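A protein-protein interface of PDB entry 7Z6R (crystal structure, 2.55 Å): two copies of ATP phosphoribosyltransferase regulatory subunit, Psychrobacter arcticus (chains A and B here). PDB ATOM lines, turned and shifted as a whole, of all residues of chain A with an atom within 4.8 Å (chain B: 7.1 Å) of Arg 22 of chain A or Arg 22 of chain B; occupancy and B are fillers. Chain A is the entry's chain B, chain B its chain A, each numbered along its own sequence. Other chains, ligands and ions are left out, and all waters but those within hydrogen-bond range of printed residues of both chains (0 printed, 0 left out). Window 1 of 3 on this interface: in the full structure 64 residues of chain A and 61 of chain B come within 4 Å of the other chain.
OE2 of Glu 19 of chain B lies within hydrogen-bond range of ND1 of His 23 of chain A, 2.6 Å away.
OE2 of Glu 19 of chain A is in hydrogen-bond range of ND1 of His 23 of chain B (2.8 Å).
The side-chain hydroxyl of Ser 38 of chain B sits at hydrogen-bond distance from the side-chain amide nitrogen of Gln 18 of chain A, at 3.4 Å.
The guanidinium group of Arg 22 of chain B lies close to the guanidinium group of Arg 22 of chain A, at 3.4 Å.
Printed residues of chain B within 4 Å of Gln 18 of chain A: Ser 38 (3.4 Å).
Arg 22 of chain A touches just one residue of chain B: Arg 22 (3.4 Å).
Printed residues of chain B within 4 Å of His 23 of chain A: Glu 19 and His 23.
Arg 22 of chain B touches one residue of chain A.
Of the printed residues of chain A, Gln 27 of chain B touches Glu 19 (3.5 Å).
Hydrophobic or aromatic side chains of chain B within 4 Å of the printed part of chain A: His 23 and Leu 36.
Along chain B the printed residues that touch a printed residue of chain A span positions 19 to 38.
Glu 19 of chain A touches His 23 of chain B, and with the chains exchanged His 23 of chain A touches Glu 19 of chain B.
Arg 22 of chain B touches its own counterpart, Arg 22 of chain A.
His 23 of chain A touches its own counterpart, His 23 of chain B.
Thr 26 of chain A touches Glu 19 of chain B, but with the chains exchanged Glu 19 of chain A does not touch Thr 26 of chain B (4.1 Å).
Of the 8 pairs that touch across the chains among the printed residues, 4 have their exchanged pair printed and touching as well.
Among the printed residues, merely in contact across the chains: Glu 19 of chain A with Gln 27 of chain B, Glu 19 of chain A with Leu 36 of chain B, His 23 of chain A with His 23 of chain B and Thr 26 of chain A with Glu 19 of chain B.
O of Arg 22 of chain B lies within hydrogen-bond range of OG1 of Thr 26 of chain B, 2.6 Å away.
The guanidinium group of Arg 22 of chain B is in hydrogen-bond range of the backbone carbonyl oxygen of Ala 100 of chain B, 3.4 Å away.
OE1 of Glu 19 of chain A lies within salt-bridge range of NH1 of Arg 22 of chain A, at 2.5 Å.
The backbone carbonyl oxygen (O) of Arg 22 of chain A is in hydrogen-bond range of the side-chain hydroxyl (OG1) of Thr 26 of chain A (2.5 Å).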
ATOM      1  N   GLN A  18     -17.083  28.367 -17.437  1.00  0.00           N
ATOM      2  CA  GLN A  18     -18.029  27.943 -18.494  1.00  0.00           C
ATOM      3  C   GLN A  18     -17.280  27.765 -19.817  1.00  0.00           C
ATOM      4  O   GLN A  18     -17.523  26.774 -20.513  1.00  0.00           O
ATOM      5  CB  GLN A  18     -19.111  28.992 -18.682  1.00  0.00           C
ATOM      6  CG  GLN A  18     -20.246  28.502 -19.575  1.00  0.00           C
ATOM      7  CD  GLN A  18     -21.295  29.577 -19.709  1.00  0.00           C
ATOM      8  OE1 GLN A  18     -22.431  29.432 -19.250  1.00  0.00           O
ATOM      9  NE2 GLN A  18     -20.876  30.697 -20.269  1.00  0.00           N
ATOM     10  N   GLU A  19     -16.408  28.708 -20.154  1.00  0.00           N
ATOM     11  CA  GLU A  19     -15.557  28.658 -21.371  1.00  0.00           C
ATOM     12  C   GLU A  19     -14.734  27.360 -21.352  1.00  0.00           C
ATOM     13  O   GLU A  19     -14.679  26.664 -22.393  1.00  0.00           O
ATOM     14  CB  GLU A  19     -14.718  29.935 -21.442  1.00  0.00           C
ATOM     15  CG  GLU A  19     -13.585  29.882 -22.442  1.00  0.00           C
ATOM     16  CD  GLU A  19     -14.054  29.619 -23.859  1.00  0.00           C
ATOM     17  OE1 GLU A  19     -15.040  30.278 -24.292  1.00  0.00           O
ATOM     18  OE2 GLU A  19     -13.455  28.734 -24.523  1.00  0.00           O
ATOM     19  N   VAL A  20     -14.144  27.026 -20.197  1.00  0.00           N
ATOM     20  CA  VAL A  20     -13.262  25.835 -20.021  1.00  0.00           C
ATOM     21  C   VAL A  20     -14.129  24.576 -20.119  1.00  0.00           C
ATOM     22  O   VAL A  20     -13.748  23.707 -20.908  1.00  0.00           O
ATOM     23  CB  VAL A  20     -12.442  25.898 -18.716  1.00  0.00           C
ATOM     24  CG1 VAL A  20     -11.895  24.534 -18.347  1.00  0.00           C
ATOM     25  CG2 VAL A  20     -11.308  26.912 -18.800  1.00  0.00           C
ATOM     26  N   LEU A  21     -15.244  24.490 -19.378  1.00  0.00           N
ATOM     27  CA  LEU A  21     -16.222  23.366 -19.500  1.00  0.00           C
ATOM     28  C   LEU A  21     -16.653  23.199 -20.963  1.00  0.00           C
ATOM     29  O   LEU A  21     -16.341  22.148 -21.540  1.00  0.00           O
ATOM     30  CB  LEU A  21     -17.466  23.620 -18.646  1.00  0.00           C
ATOM     31  CG  LEU A  21     -17.269  23.669 -17.138  1.00  0.00           C
ATOM     32  CD1 LEU A  21     -18.619  23.615 -16.434  1.00  0.00           C
ATOM     33  CD2 LEU A  21     -16.363  22.540 -16.666  1.00  0.00           C
ATOM     34  N   ARG A  22     -17.354  24.192 -21.531  1.00  0.00           N
ATOM     35  CA  ARG A  22     -17.879  24.153 -22.925  1.00  0.00           C
ATOM     36  C   ARG A  22     -16.809  23.526 -23.827  1.00  0.00           C
ATOM     37  O   ARG A  22     -17.161  22.609 -24.601  1.00  0.00           O
ATOM     38  CB  ARG A  22     -18.286  25.554 -23.396  1.00  0.00           C
ATOM     39  CG  ARG A  22     -18.924  25.617 -24.776  1.00  0.00           C
ATOM     40  CD  ARG A  22     -19.574  26.966 -25.057  1.00  0.00           C
ATOM     41  NE  ARG A  22     -18.621  28.080 -25.166  1.00  0.00           N
ATOM     42  CZ  ARG A  22     -18.433  29.081 -24.279  1.00  0.00           C
ATOM     43  NH1 ARG A  22     -17.517  30.004 -24.526  1.00  0.00           N
ATOM     44  NH2 ARG A  22     -19.130  29.177 -23.156  1.00  0.00           N
ATOM     45  N   HIS A  23     -15.550  23.952 -23.683  1.00  0.00           N
ATOM     46  CA  HIS A  23     -14.436  23.557 -24.584  1.00  0.00           C
ATOM     47  C   HIS A  23     -13.945  22.130 -24.284  1.00  0.00           C
ATOM     48  O   HIS A  23     -13.723  21.386 -25.247  1.00  0.00           O
ATOM     49  CB  HIS A  23     -13.298  24.573 -24.514  1.00  0.00           C
ATOM     50  CG  HIS A  23     -12.147  24.176 -25.372  1.00  0.00           C
ATOM     51  ND1 HIS A  23     -12.157  24.354 -26.738  1.00  0.00           N
ATOM     52  CD2 HIS A  23     -10.969  23.585 -25.075  1.00  0.00           C
ATOM     53  CE1 HIS A  23     -11.031  23.892 -27.248  1.00  0.00           C
ATOM     54  NE2 HIS A  23     -10.284  23.414 -26.248  1.00  0.00           N
ATOM     55  N   GLN A  24     -13.728  21.770 -23.013  1.00  0.00           N
ATOM     56  CA  GLN A  24     -13.174  20.450 -22.616  1.00  0.00           C
ATOM     57  C   GLN A  24     -14.161  19.349 -23.019  1.00  0.00           C
ATOM     58  O   GLN A  24     -13.741  18.344 -23.605  1.00  0.00           O
ATOM     59  CB  GLN A  24     -12.945  20.362 -21.107  1.00  0.00           C
ATOM     60  CG  GLN A  24     -11.872  21.282 -20.543  1.00  0.00           C
ATOM     61  CD  GLN A  24     -10.509  21.142 -21.179  1.00  0.00           C
ATOM     62  OE1 GLN A  24     -10.340  21.402 -22.373  1.00  0.00           O
ATOM     63  NE2 GLN A  24      -9.519  20.761 -20.375  1.00  0.00           N
ATOM     64  N   LEU A  25     -15.434  19.542 -22.692  1.00  0.00           N
ATOM     65  CA  LEU A  25     -16.540  18.618 -23.042  1.00  0.00           C
ATOM     66  C   LEU A  25     -16.679  18.507 -24.569  1.00  0.00           C
ATOM     67  O   LEU A  25     -16.920  17.411 -25.046  1.00  0.00           O
ATOM     68  CB  LEU A  25     -17.830  19.131 -22.409  1.00  0.00           C
ATOM     69  CG  LEU A  25     -17.850  19.176 -20.887  1.00  0.00           C
ATOM     70  CD1 LEU A  25     -19.158  19.753 -20.392  1.00  0.00           C
ATOM     71  CD2 LEU A  25     -17.652  17.798 -20.299  1.00  0.00           C
ATOM     72  N   THR A  26     -16.520  19.590 -25.321  1.00  0.00           N
ATOM     73  CA  THR A  26     -16.629  19.561 -26.796  1.00  0.00           C
ATOM     74  C   THR A  26     -15.518  18.672 -27.361  1.00  0.00           C
ATOM     75  O   THR A  26     -15.847  17.772 -28.158  1.00  0.00           O
ATOM     76  CB  THR A  26     -16.650  20.981 -27.367  1.00  0.00           C
ATOM     77  OG1 THR A  26     -17.825  21.581 -26.828  1.00  0.00           O
ATOM     78  CG2 THR A  26     -16.664  21.023 -28.879  1.00  0.00           C
ATOM     79  N   ALA A 100     -22.728  22.168 -28.973  1.00  0.00           N
ATOM     80  CA  ALA A 100     -22.896  23.038 -27.795  1.00  0.00           C
ATOM     81  C   ALA A 100     -23.328  24.393 -28.318  1.00  0.00           C
ATOM     82  O   ALA A 100     -22.669  24.863 -29.257  1.00  0.00           O
ATOM     83  CB  ALA A 100     -21.601  23.125 -27.032  1.00  0.00           C
ATOM     84  N   LEU A 118     -27.231  26.718 -21.797  1.00  0.00           N
ATOM     85  CA  LEU A 118     -26.151  26.413 -22.761  1.00  0.00           C
ATOM     86  C   LEU A 118     -26.224  24.916 -23.027  1.00  0.00           C
ATOM     87  O   LEU A 118     -25.817  24.142 -22.143  1.00  0.00           O
ATOM     88  CB  LEU A 118     -24.813  26.844 -22.158  1.00  0.00           C
ATOM     89  CG  LEU A 118     -23.586  26.562 -23.014  1.00  0.00           C
ATOM     90  CD1 LEU A 118     -23.849  26.948 -24.458  1.00  0.00           C
ATOM     91  CD2 LEU A 118     -22.365  27.286 -22.453  1.00  0.00           C
ATOM     92  N   LEU A 120     -25.535  21.350 -24.446  1.00  0.00           N
ATOM     93  CA  LEU A 120     -24.440  20.481 -24.947  1.00  0.00           C
ATOM     94  C   LEU A 120     -24.976  19.059 -25.073  1.00  0.00           C
ATOM     95  O   LEU A 120     -25.688  18.619 -24.157  1.00  0.00           O
ATOM     96  CB  LEU A 120     -23.277  20.555 -23.955  1.00  0.00           C
ATOM     97  CG  LEU A 120     -21.956  19.959 -24.437  1.00  0.00           C
ATOM     98  CD1 LEU A 120     -20.777  20.864 -24.095  1.00  0.00           C
ATOM     99  CD2 LEU A 120     -21.760  18.587 -23.838  1.00  0.00           C
ATOM    100  N   VAL A 312     -24.953  23.001 -19.743  1.00  0.00           N
ATOM    101  CA  VAL A 312     -23.546  23.151 -19.268  1.00  0.00           C
ATOM    102  C   VAL A 312     -23.518  24.149 -18.109  1.00  0.00           C
ATOM    103  O   VAL A 312     -22.729  23.949 -17.195  1.00  0.00           O
ATOM    104  CB  VAL A 312     -22.611  23.593 -20.408  1.00  0.00           C
ATOM    105  CG1 VAL A 312     -21.213  23.931 -19.916  1.00  0.00           C
ATOM    106  CG2 VAL A 312     -22.531  22.527 -21.477  1.00  0.00           C
ATOM    107  N   HIS B  16     -15.534  22.494 -35.821  1.00  0.00           N
ATOM    108  CA  HIS B  16     -14.332  22.194 -35.014  1.00  0.00           C
ATOM    109  C   HIS B  16     -13.357  23.371 -35.098  1.00  0.00           C
ATOM    110  O   HIS B  16     -12.749  23.706 -34.079  1.00  0.00           O
ATOM    111  CB  HIS B  16     -13.666  20.893 -35.477  1.00  0.00           C
ATOM    112  CG  HIS B  16     -12.316  20.727 -34.861  1.00  0.00           C
ATOM    113  ND1 HIS B  16     -12.148  20.565 -33.495  1.00  0.00           N
ATOM    114  CD2 HIS B  16     -11.077  20.791 -35.400  1.00  0.00           C
ATOM    115  CE1 HIS B  16     -10.866  20.467 -33.231  1.00  0.00           C
ATOM    116  NE2 HIS B  16     -10.189  20.600 -34.384  1.00  0.00           N
ATOM    117  N   LYS B  17     -13.192  23.948 -36.283  1.00  0.00           N
ATOM    118  CA  LYS B  17     -12.225  25.045 -36.534  1.00  0.00           C
ATOM    119  C   LYS B  17     -12.716  26.321 -35.838  1.00  0.00           C
ATOM    120  O   LYS B  17     -11.898  26.999 -35.193  1.00  0.00           O
ATOM    121  CB  LYS B  17     -12.059  25.240 -38.034  1.00  0.00           C
ATOM    122  CG  LYS B  17     -10.915  26.153 -38.443  1.00  0.00           C
ATOM    123  CD  LYS B  17     -11.138  26.762 -39.805  1.00  0.00           C
ATOM    124  CE  LYS B  17     -10.589  25.907 -40.922  1.00  0.00           C
ATOM    125  NZ  LYS B  17     -11.038  26.418 -42.231  1.00  0.00           N
ATOM    126  N   GLN B  18     -14.004  26.629 -35.946  1.00  0.00           N
ATOM    127  CA  GLN B  18     -14.631  27.752 -35.215  1.00  0.00           C
ATOM    128  C   GLN B  18     -14.448  27.565 -33.709  1.00  0.00           C
ATOM    129  O   GLN B  18     -14.108  28.551 -33.033  1.00  0.00           O
ATOM    130  CB  GLN B  18     -16.113  27.819 -35.536  1.00  0.00           C
ATOM    131  CG  GLN B  18     -16.793  29.021 -34.916  1.00  0.00           C
ATOM    132  CD  GLN B  18     -18.219  29.076 -35.380  1.00  0.00           C
ATOM    133  OE1 GLN B  18     -18.638  30.086 -35.918  1.00  0.00           O
ATOM    134  NE2 GLN B  18     -18.945  27.983 -35.191  1.00  0.00           N
ATOM    135  N   GLU B  19     -14.708  26.360 -33.205  1.00  0.00           N
ATOM    136  CA  GLU B  19     -14.559  25.997 -31.772  1.00  0.00           C
ATOM    137  C   GLU B  19     -13.108  26.305 -31.358  1.00  0.00           C
ATOM    138  O   GLU B  19     -12.916  26.924 -30.292  1.00  0.00           O
ATOM    139  CB  GLU B  19     -14.968  24.531 -31.590  1.00  0.00           C
ATOM    140  CG  GLU B  19     -14.512  23.906 -30.284  1.00  0.00           C
ATOM    141  CD  GLU B  19     -15.046  24.627 -29.062  1.00  0.00           C
ATOM    142  OE1 GLU B  19     -16.259  24.897 -29.034  1.00  0.00           O
ATOM    143  OE2 GLU B  19     -14.243  24.949 -28.158  1.00  0.00           O
ATOM    144  N   VAL B  20     -12.133  25.920 -32.191  1.00  0.00           N
ATOM    145  CA  VAL B  20     -10.681  26.097 -31.919  1.00  0.00           C
ATOM    146  C   VAL B  20     -10.343  27.594 -31.954  1.00  0.00           C
ATOM    147  O   VAL B  20      -9.725  28.053 -30.991  1.00  0.00           O
ATOM    148  CB  VAL B  20      -9.805  25.276 -32.882  1.00  0.00           C
ATOM    149  CG1 VAL B  20      -8.359  25.750 -32.864  1.00  0.00           C
ATOM    150  CG2 VAL B  20      -9.866  23.795 -32.552  1.00  0.00           C
ATOM    151  N   LEU B  21     -10.735  28.320 -33.007  1.00  0.00           N
ATOM    152  CA  LEU B  21     -10.544  29.794 -33.096  1.00  0.00           C
ATOM    153  C   LEU B  21     -11.168  30.466 -31.871  1.00  0.00           C
ATOM    154  O   LEU B  21     -10.428  31.083 -31.103  1.00  0.00           O
ATOM    155  CB  LEU B  21     -11.176  30.364 -34.368  1.00  0.00           C
ATOM    156  CG  LEU B  21     -10.555  29.912 -35.687  1.00  0.00           C
ATOM    157  CD1 LEU B  21     -11.012  30.821 -36.812  1.00  0.00           C
ATOM    158  CD2 LEU B  21      -9.034  29.864 -35.619  1.00  0.00           C
ATOM    159  N   ARG B  22     -12.484  30.364 -31.712  1.00  0.00           N
ATOM    160  CA  ARG B  22     -13.234  31.022 -30.611  1.00  0.00           C
ATOM    161  C   ARG B  22     -12.437  30.830 -29.315  1.00  0.00           C
ATOM    162  O   ARG B  22     -12.274  31.822 -28.578  1.00  0.00           O
ATOM    163  CB  ARG B  22     -14.652  30.448 -30.499  1.00  0.00           C
ATOM    164  CG  ARG B  22     -15.543  31.194 -29.518  1.00  0.00           C
ATOM    165  CD  ARG B  22     -16.486  30.244 -28.819  1.00  0.00           C
ATOM    166  NE  ARG B  22     -17.319  30.934 -27.855  1.00  0.00           N
ATOM    167  CZ  ARG B  22     -18.649  30.918 -27.834  1.00  0.00           C
ATOM    168  NH1 ARG B  22     -19.338  30.238 -28.741  1.00  0.00           N
ATOM    169  NH2 ARG B  22     -19.295  31.601 -26.901  1.00  0.00           N
ATOM    170  N   HIS B  23     -11.920  29.618 -29.076  1.00  0.00           N
ATOM    171  CA  HIS B  23     -11.227  29.244 -27.812  1.00  0.00           C
ATOM    172  C   HIS B  23      -9.818  29.853 -27.744  1.00  0.00           C
ATOM    173  O   HIS B  23      -9.496  30.406 -26.683  1.00  0.00           O
ATOM    174  CB  HIS B  23     -11.185  27.724 -27.613  1.00  0.00           C
ATOM    175  CG  HIS B  23     -10.459  27.349 -26.372  1.00  0.00           C
ATOM    176  ND1 HIS B  23     -11.029  27.489 -25.116  1.00  0.00           N
ATOM    177  CD2 HIS B  23      -9.195  26.909 -26.179  1.00  0.00           C
ATOM    178  CE1 HIS B  23     -10.153  27.128 -24.198  1.00  0.00           C
ATOM    179  NE2 HIS B  23      -9.017  26.765 -24.826  1.00  0.00           N
ATOM    180  N   GLN B  24      -9.002  29.727 -28.801  1.00  0.00           N
ATOM    181  CA  GLN B  24      -7.597  30.214 -28.824  1.00  0.00           C
ATOM    182  C   GLN B  24      -7.594  31.729 -28.609  1.00  0.00           C
ATOM    183  O   GLN B  24      -6.808  32.212 -27.768  1.00  0.00           O
ATOM    184  CB  GLN B  24      -6.877  29.914 -30.144  1.00  0.00           C
ATOM    185  CG  GLN B  24      -6.691  28.441 -30.507  1.00  0.00           C
ATOM    186  CD  GLN B  24      -6.096  27.520 -29.460  1.00  0.00           C
ATOM    187  OE1 GLN B  24      -6.118  27.781 -28.255  1.00  0.00           O
ATOM    188  NE2 GLN B  24      -5.618  26.370 -29.919  1.00  0.00           N
ATOM    189  N   LEU B  25      -8.431  32.447 -29.361  1.00  0.00           N
ATOM    190  CA  LEU B  25      -8.570  33.922 -29.288  1.00  0.00           C
ATOM    191  C   LEU B  25      -9.070  34.349 -27.904  1.00  0.00           C
ATOM    192  O   LEU B  25      -8.603  35.370 -27.400  1.00  0.00           O
ATOM    193  CB  LEU B  25      -9.529  34.367 -30.390  1.00  0.00           C
ATOM    194  CG  LEU B  25      -9.018  34.120 -31.806  1.00  0.00           C
ATOM    195  CD1 LEU B  25     -10.073  34.504 -32.831  1.00  0.00           C
ATOM    196  CD2 LEU B  25      -7.728  34.884 -32.055  1.00  0.00           C
ATOM    197  N   THR B  26      -9.986  33.605 -27.297  1.00  0.00           N
ATOM    198  CA  THR B  26     -10.534  33.951 -25.960  1.00  0.00           C
ATOM    199  C   THR B  26      -9.400  33.867 -24.932  1.00  0.00           C
ATOM    200  O   THR B  26      -9.220  34.825 -24.177  1.00  0.00           O
ATOM    201  CB  THR B  26     -11.757  33.081 -25.660  1.00  0.00           C
ATOM    202  OG1 THR B  26     -12.729  33.450 -26.643  1.00  0.00           O
ATOM    203  CG2 THR B  26     -12.305  33.269 -24.263  1.00  0.00           C
ATOM    204  N   GLN B  27      -8.646  32.772 -24.910  1.00  0.00           N
ATOM    205  CA  GLN B  27      -7.575  32.570 -23.904  1.00  0.00           C
ATOM    206  C   GLN B  27      -6.436  33.569 -24.179  1.00  0.00           C
ATOM    207  O   GLN B  27      -5.828  34.039 -23.199  1.00  0.00           O
ATOM    208  CB  GLN B  27      -7.129  31.108 -23.850  1.00  0.00           C
ATOM    209  CG  GLN B  27      -8.239  30.163 -23.406  1.00  0.00           C
ATOM    210  CD  GLN B  27      -8.831  30.429 -22.036  1.00  0.00           C
ATOM    211  OE1 GLN B  27      -8.139  30.791 -21.086  1.00  0.00           O
ATOM    212  NE2 GLN B  27     -10.137  30.237 -21.918  1.00  0.00           N
ATOM    213  N   LEU B  36     -12.964  37.836 -19.068  1.00  0.00           N
ATOM    214  CA  LEU B  36     -14.055  37.216 -19.852  1.00  0.00           C
ATOM    215  C   LEU B  36     -15.380  37.529 -19.153  1.00  0.00           C
ATOM    216  O   LEU B  36     -15.483  37.324 -17.926  1.00  0.00           O
ATOM    217  CB  LEU B  36     -13.813  35.710 -19.973  1.00  0.00           C
ATOM    218  CG  LEU B  36     -14.819  34.943 -20.837  1.00  0.00           C
ATOM    219  CD1 LEU B  36     -14.982  35.576 -22.219  1.00  0.00           C
ATOM    220  CD2 LEU B  36     -14.385  33.490 -20.979  1.00  0.00           C
ATOM    221  N   SER B  38     -19.699  36.871 -19.944  1.00  0.00           N
ATOM    222  CA  SER B  38     -20.655  36.108 -20.782  1.00  0.00           C
ATOM    223  C   SER B  38     -22.055  36.624 -20.480  1.00  0.00           C
ATOM    224  O   SER B  38     -22.794  36.028 -19.707  1.00  0.00           O
ATOM    225  CB  SER B  38     -20.503  34.626 -20.522  1.00  0.00           C
ATOM    226  OG  SER B  38     -21.101  33.859 -21.556  1.00  0.00           O
ATOM    227  N   ARG B  75     -30.070  40.290 -28.503  1.00  0.00           N
ATOM    228  CA  ARG B  75     -28.949  41.224 -28.748  1.00  0.00           C
ATOM    229  C   ARG B  75     -28.447  41.062 -30.187  1.00  0.00           C
ATOM    230  O   ARG B  75     -28.264  39.898 -30.641  1.00  0.00           O
ATOM    231  CB  ARG B  75     -27.834  40.960 -27.736  1.00  0.00           C
ATOM    232  CG  ARG B  75     -27.112  39.642 -27.965  1.00  0.00           C
ATOM    233  CD  ARG B  75     -26.257  39.291 -26.782  1.00  0.00           C
ATOM    234  NE  ARG B  75     -25.476  38.104 -27.072  1.00  0.00           N
ATOM    235  CZ  ARG B  75     -24.584  37.570 -26.257  1.00  0.00           C
ATOM    236  NH1 ARG B  75     -24.342  38.118 -25.078  1.00  0.00           N
ATOM    237  NH2 ARG B  75     -23.928  36.492 -26.636  1.00  0.00           N
ATOM    238  N   TYR B  99     -15.028  39.088 -24.548  1.00  0.00           N
ATOM    239  CA  TYR B  99     -16.286  38.326 -24.679  1.00  0.00           C
ATOM    240  C   TYR B  99     -16.312  37.662 -26.053  1.00  0.00           C
ATOM    241  O   TYR B  99     -15.694  38.170 -27.007  1.00  0.00           O
ATOM    242  CB  TYR B  99     -17.473  39.267 -24.503  1.00  0.00           C
ATOM    243  CG  TYR B  99     -17.497  40.329 -25.566  1.00  0.00           C
ATOM    244  CD1 TYR B  99     -18.041  40.066 -26.811  1.00  0.00           C
ATOM    245  CD2 TYR B  99     -16.903  41.564 -25.360  1.00  0.00           C
ATOM    246  CE1 TYR B  99     -18.021  41.016 -27.814  1.00  0.00           C
ATOM    247  CE2 TYR B  99     -16.888  42.529 -26.351  1.00  0.00           C
ATOM    248  CZ  TYR B  99     -17.448  42.252 -27.583  1.00  0.00           C
ATOM    249  OH  TYR B  99     -17.451  43.185 -28.582  1.00  0.00           O
ATOM    250  N   ALA B 100     -17.014  36.539 -26.127  1.00  0.00           N
ATOM    251  CA  ALA B 100     -17.415  35.885 -27.384  1.00  0.00           C
ATOM    252  C   ALA B 100     -18.849  35.402 -27.192  1.00  0.00           C
ATOM    253  O   ALA B 100     -19.187  34.946 -26.098  1.00  0.00           O
ATOM    254  CB  ALA B 100     -16.464  34.772 -27.733  1.00  0.00           C
ATOM    255  N   GLY B 101     -19.685  35.575 -28.200  1.00  0.00           N
ATOM    256  CA  GLY B 101     -21.124  35.323 -28.052  1.00  0.00           C
ATOM    257  C   GLY B 101     -21.827  35.413 -29.377  1.00  0.00           C
ATOM    258  O   GLY B 101     -21.348  36.127 -30.264  1.00  0.00           O
ATOM    259  N   ASP B 102     -22.920  34.678 -29.510  1.00  0.00           N
ATOM    260  CA  ASP B 102     -23.808  34.757 -30.691  1.00  0.00           C
ATOM    261  C   ASP B 102     -24.592  36.065 -30.575  1.00  0.00           C
ATOM    262  O   ASP B 102     -25.043  36.395 -29.471  1.00  0.00           O
ATOM    263  CB  ASP B 102     -24.667  33.495 -30.802  1.00  0.00           C
ATOM    264  CG  ASP B 102     -23.912  32.254 -31.254  1.00  0.00           C
ATOM    265  OD1 ASP B 102     -22.993  32.359 -32.088  1.00  0.00           O
ATOM    266  OD2 ASP B 102     -24.275  31.173 -30.789  1.00  0.00           O
ATOM    267  N   LEU B 118     -20.811  35.344 -34.965  1.00  0.00           N
ATOM    268  CA  LEU B 118     -20.201  34.963 -33.663  1.00  0.00           C
ATOM    269  C   LEU B 118     -19.268  36.115 -33.256  1.00  0.00           C
ATOM    270  O   LEU B 118     -18.179  36.229 -33.850  1.00  0.00           O
ATOM    271  CB  LEU B 118     -19.459  33.635 -33.835  1.00  0.00           C
ATOM    272  CG  LEU B 118     -18.756  33.121 -32.593  1.00  0.00           C
ATOM    273  CD1 LEU B 118     -19.664  33.250 -31.381  1.00  0.00           C
ATOM    274  CD2 LEU B 118     -18.307  31.678 -32.778  1.00  0.00           C
ATOM    275  N   GLN B 119     -19.727  36.975 -32.346  1.00  0.00           N
ATOM    276  CA  GLN B 119     -19.059  38.261 -32.030  1.00  0.00           C
ATOM    277  C   GLN B 119     -18.032  38.025 -30.917  1.00  0.00           C
ATOM    278  O   GLN B 119     -18.431  37.615 -29.809  1.00  0.00           O
ATOM    279  CB  GLN B 119     -20.072  39.349 -31.643  1.00  0.00           C
ATOM    280  CG  GLN B 119     -19.483  40.752 -31.710  1.00  0.00           C
ATOM    281  CD  GLN B 119     -20.304  41.830 -31.046  1.00  0.00           C
ATOM    282  OE1 GLN B 119     -21.483  41.667 -30.748  1.00  0.00           O
ATOM    283  NE2 GLN B 119     -19.672  42.970 -30.821  1.00  0.00           N
ATOM    284  N   LEU B 120     -16.763  38.285 -31.226  1.00  0.00           N
ATOM    285  CA  LEU B 120     -15.622  38.260 -30.282  1.00  0.00           C
ATOM    286  C   LEU B 120     -15.037  39.672 -30.175  1.00  0.00           C
ATOM    287  O   LEU B 120     -14.892  40.330 -31.219  1.00  0.00           O
ATOM    288  CB  LEU B 120     -14.587  37.283 -30.837  1.00  0.00           C
ATOM    289  CG  LEU B 120     -13.470  36.887 -29.877  1.00  0.00           C
ATOM    290  CD1 LEU B 120     -13.187  35.402 -30.005  1.00  0.00           C
ATOM    291  CD2 LEU B 120     -12.204  37.691 -30.124  1.00  0.00           C
ATOM    292  N   VAL B 312     -16.102  35.966 -35.685  1.00  0.00           N
ATOM    293  CA  VAL B 312     -15.158  34.809 -35.687  1.00  0.00           C
ATOM    294  C   VAL B 312     -15.458  33.918 -36.893  1.00  0.00           C
ATOM    295  O   VAL B 312     -14.498  33.388 -37.481  1.00  0.00           O
ATOM    296  CB  VAL B 312     -15.219  34.030 -34.364  1.00  0.00           C
ATOM    297  CG1 VAL B 312     -14.398  32.746 -34.427  1.00  0.00           C
ATOM    298  CG2 VAL B 312     -14.755  34.892 -33.195  1.00  0.00           C
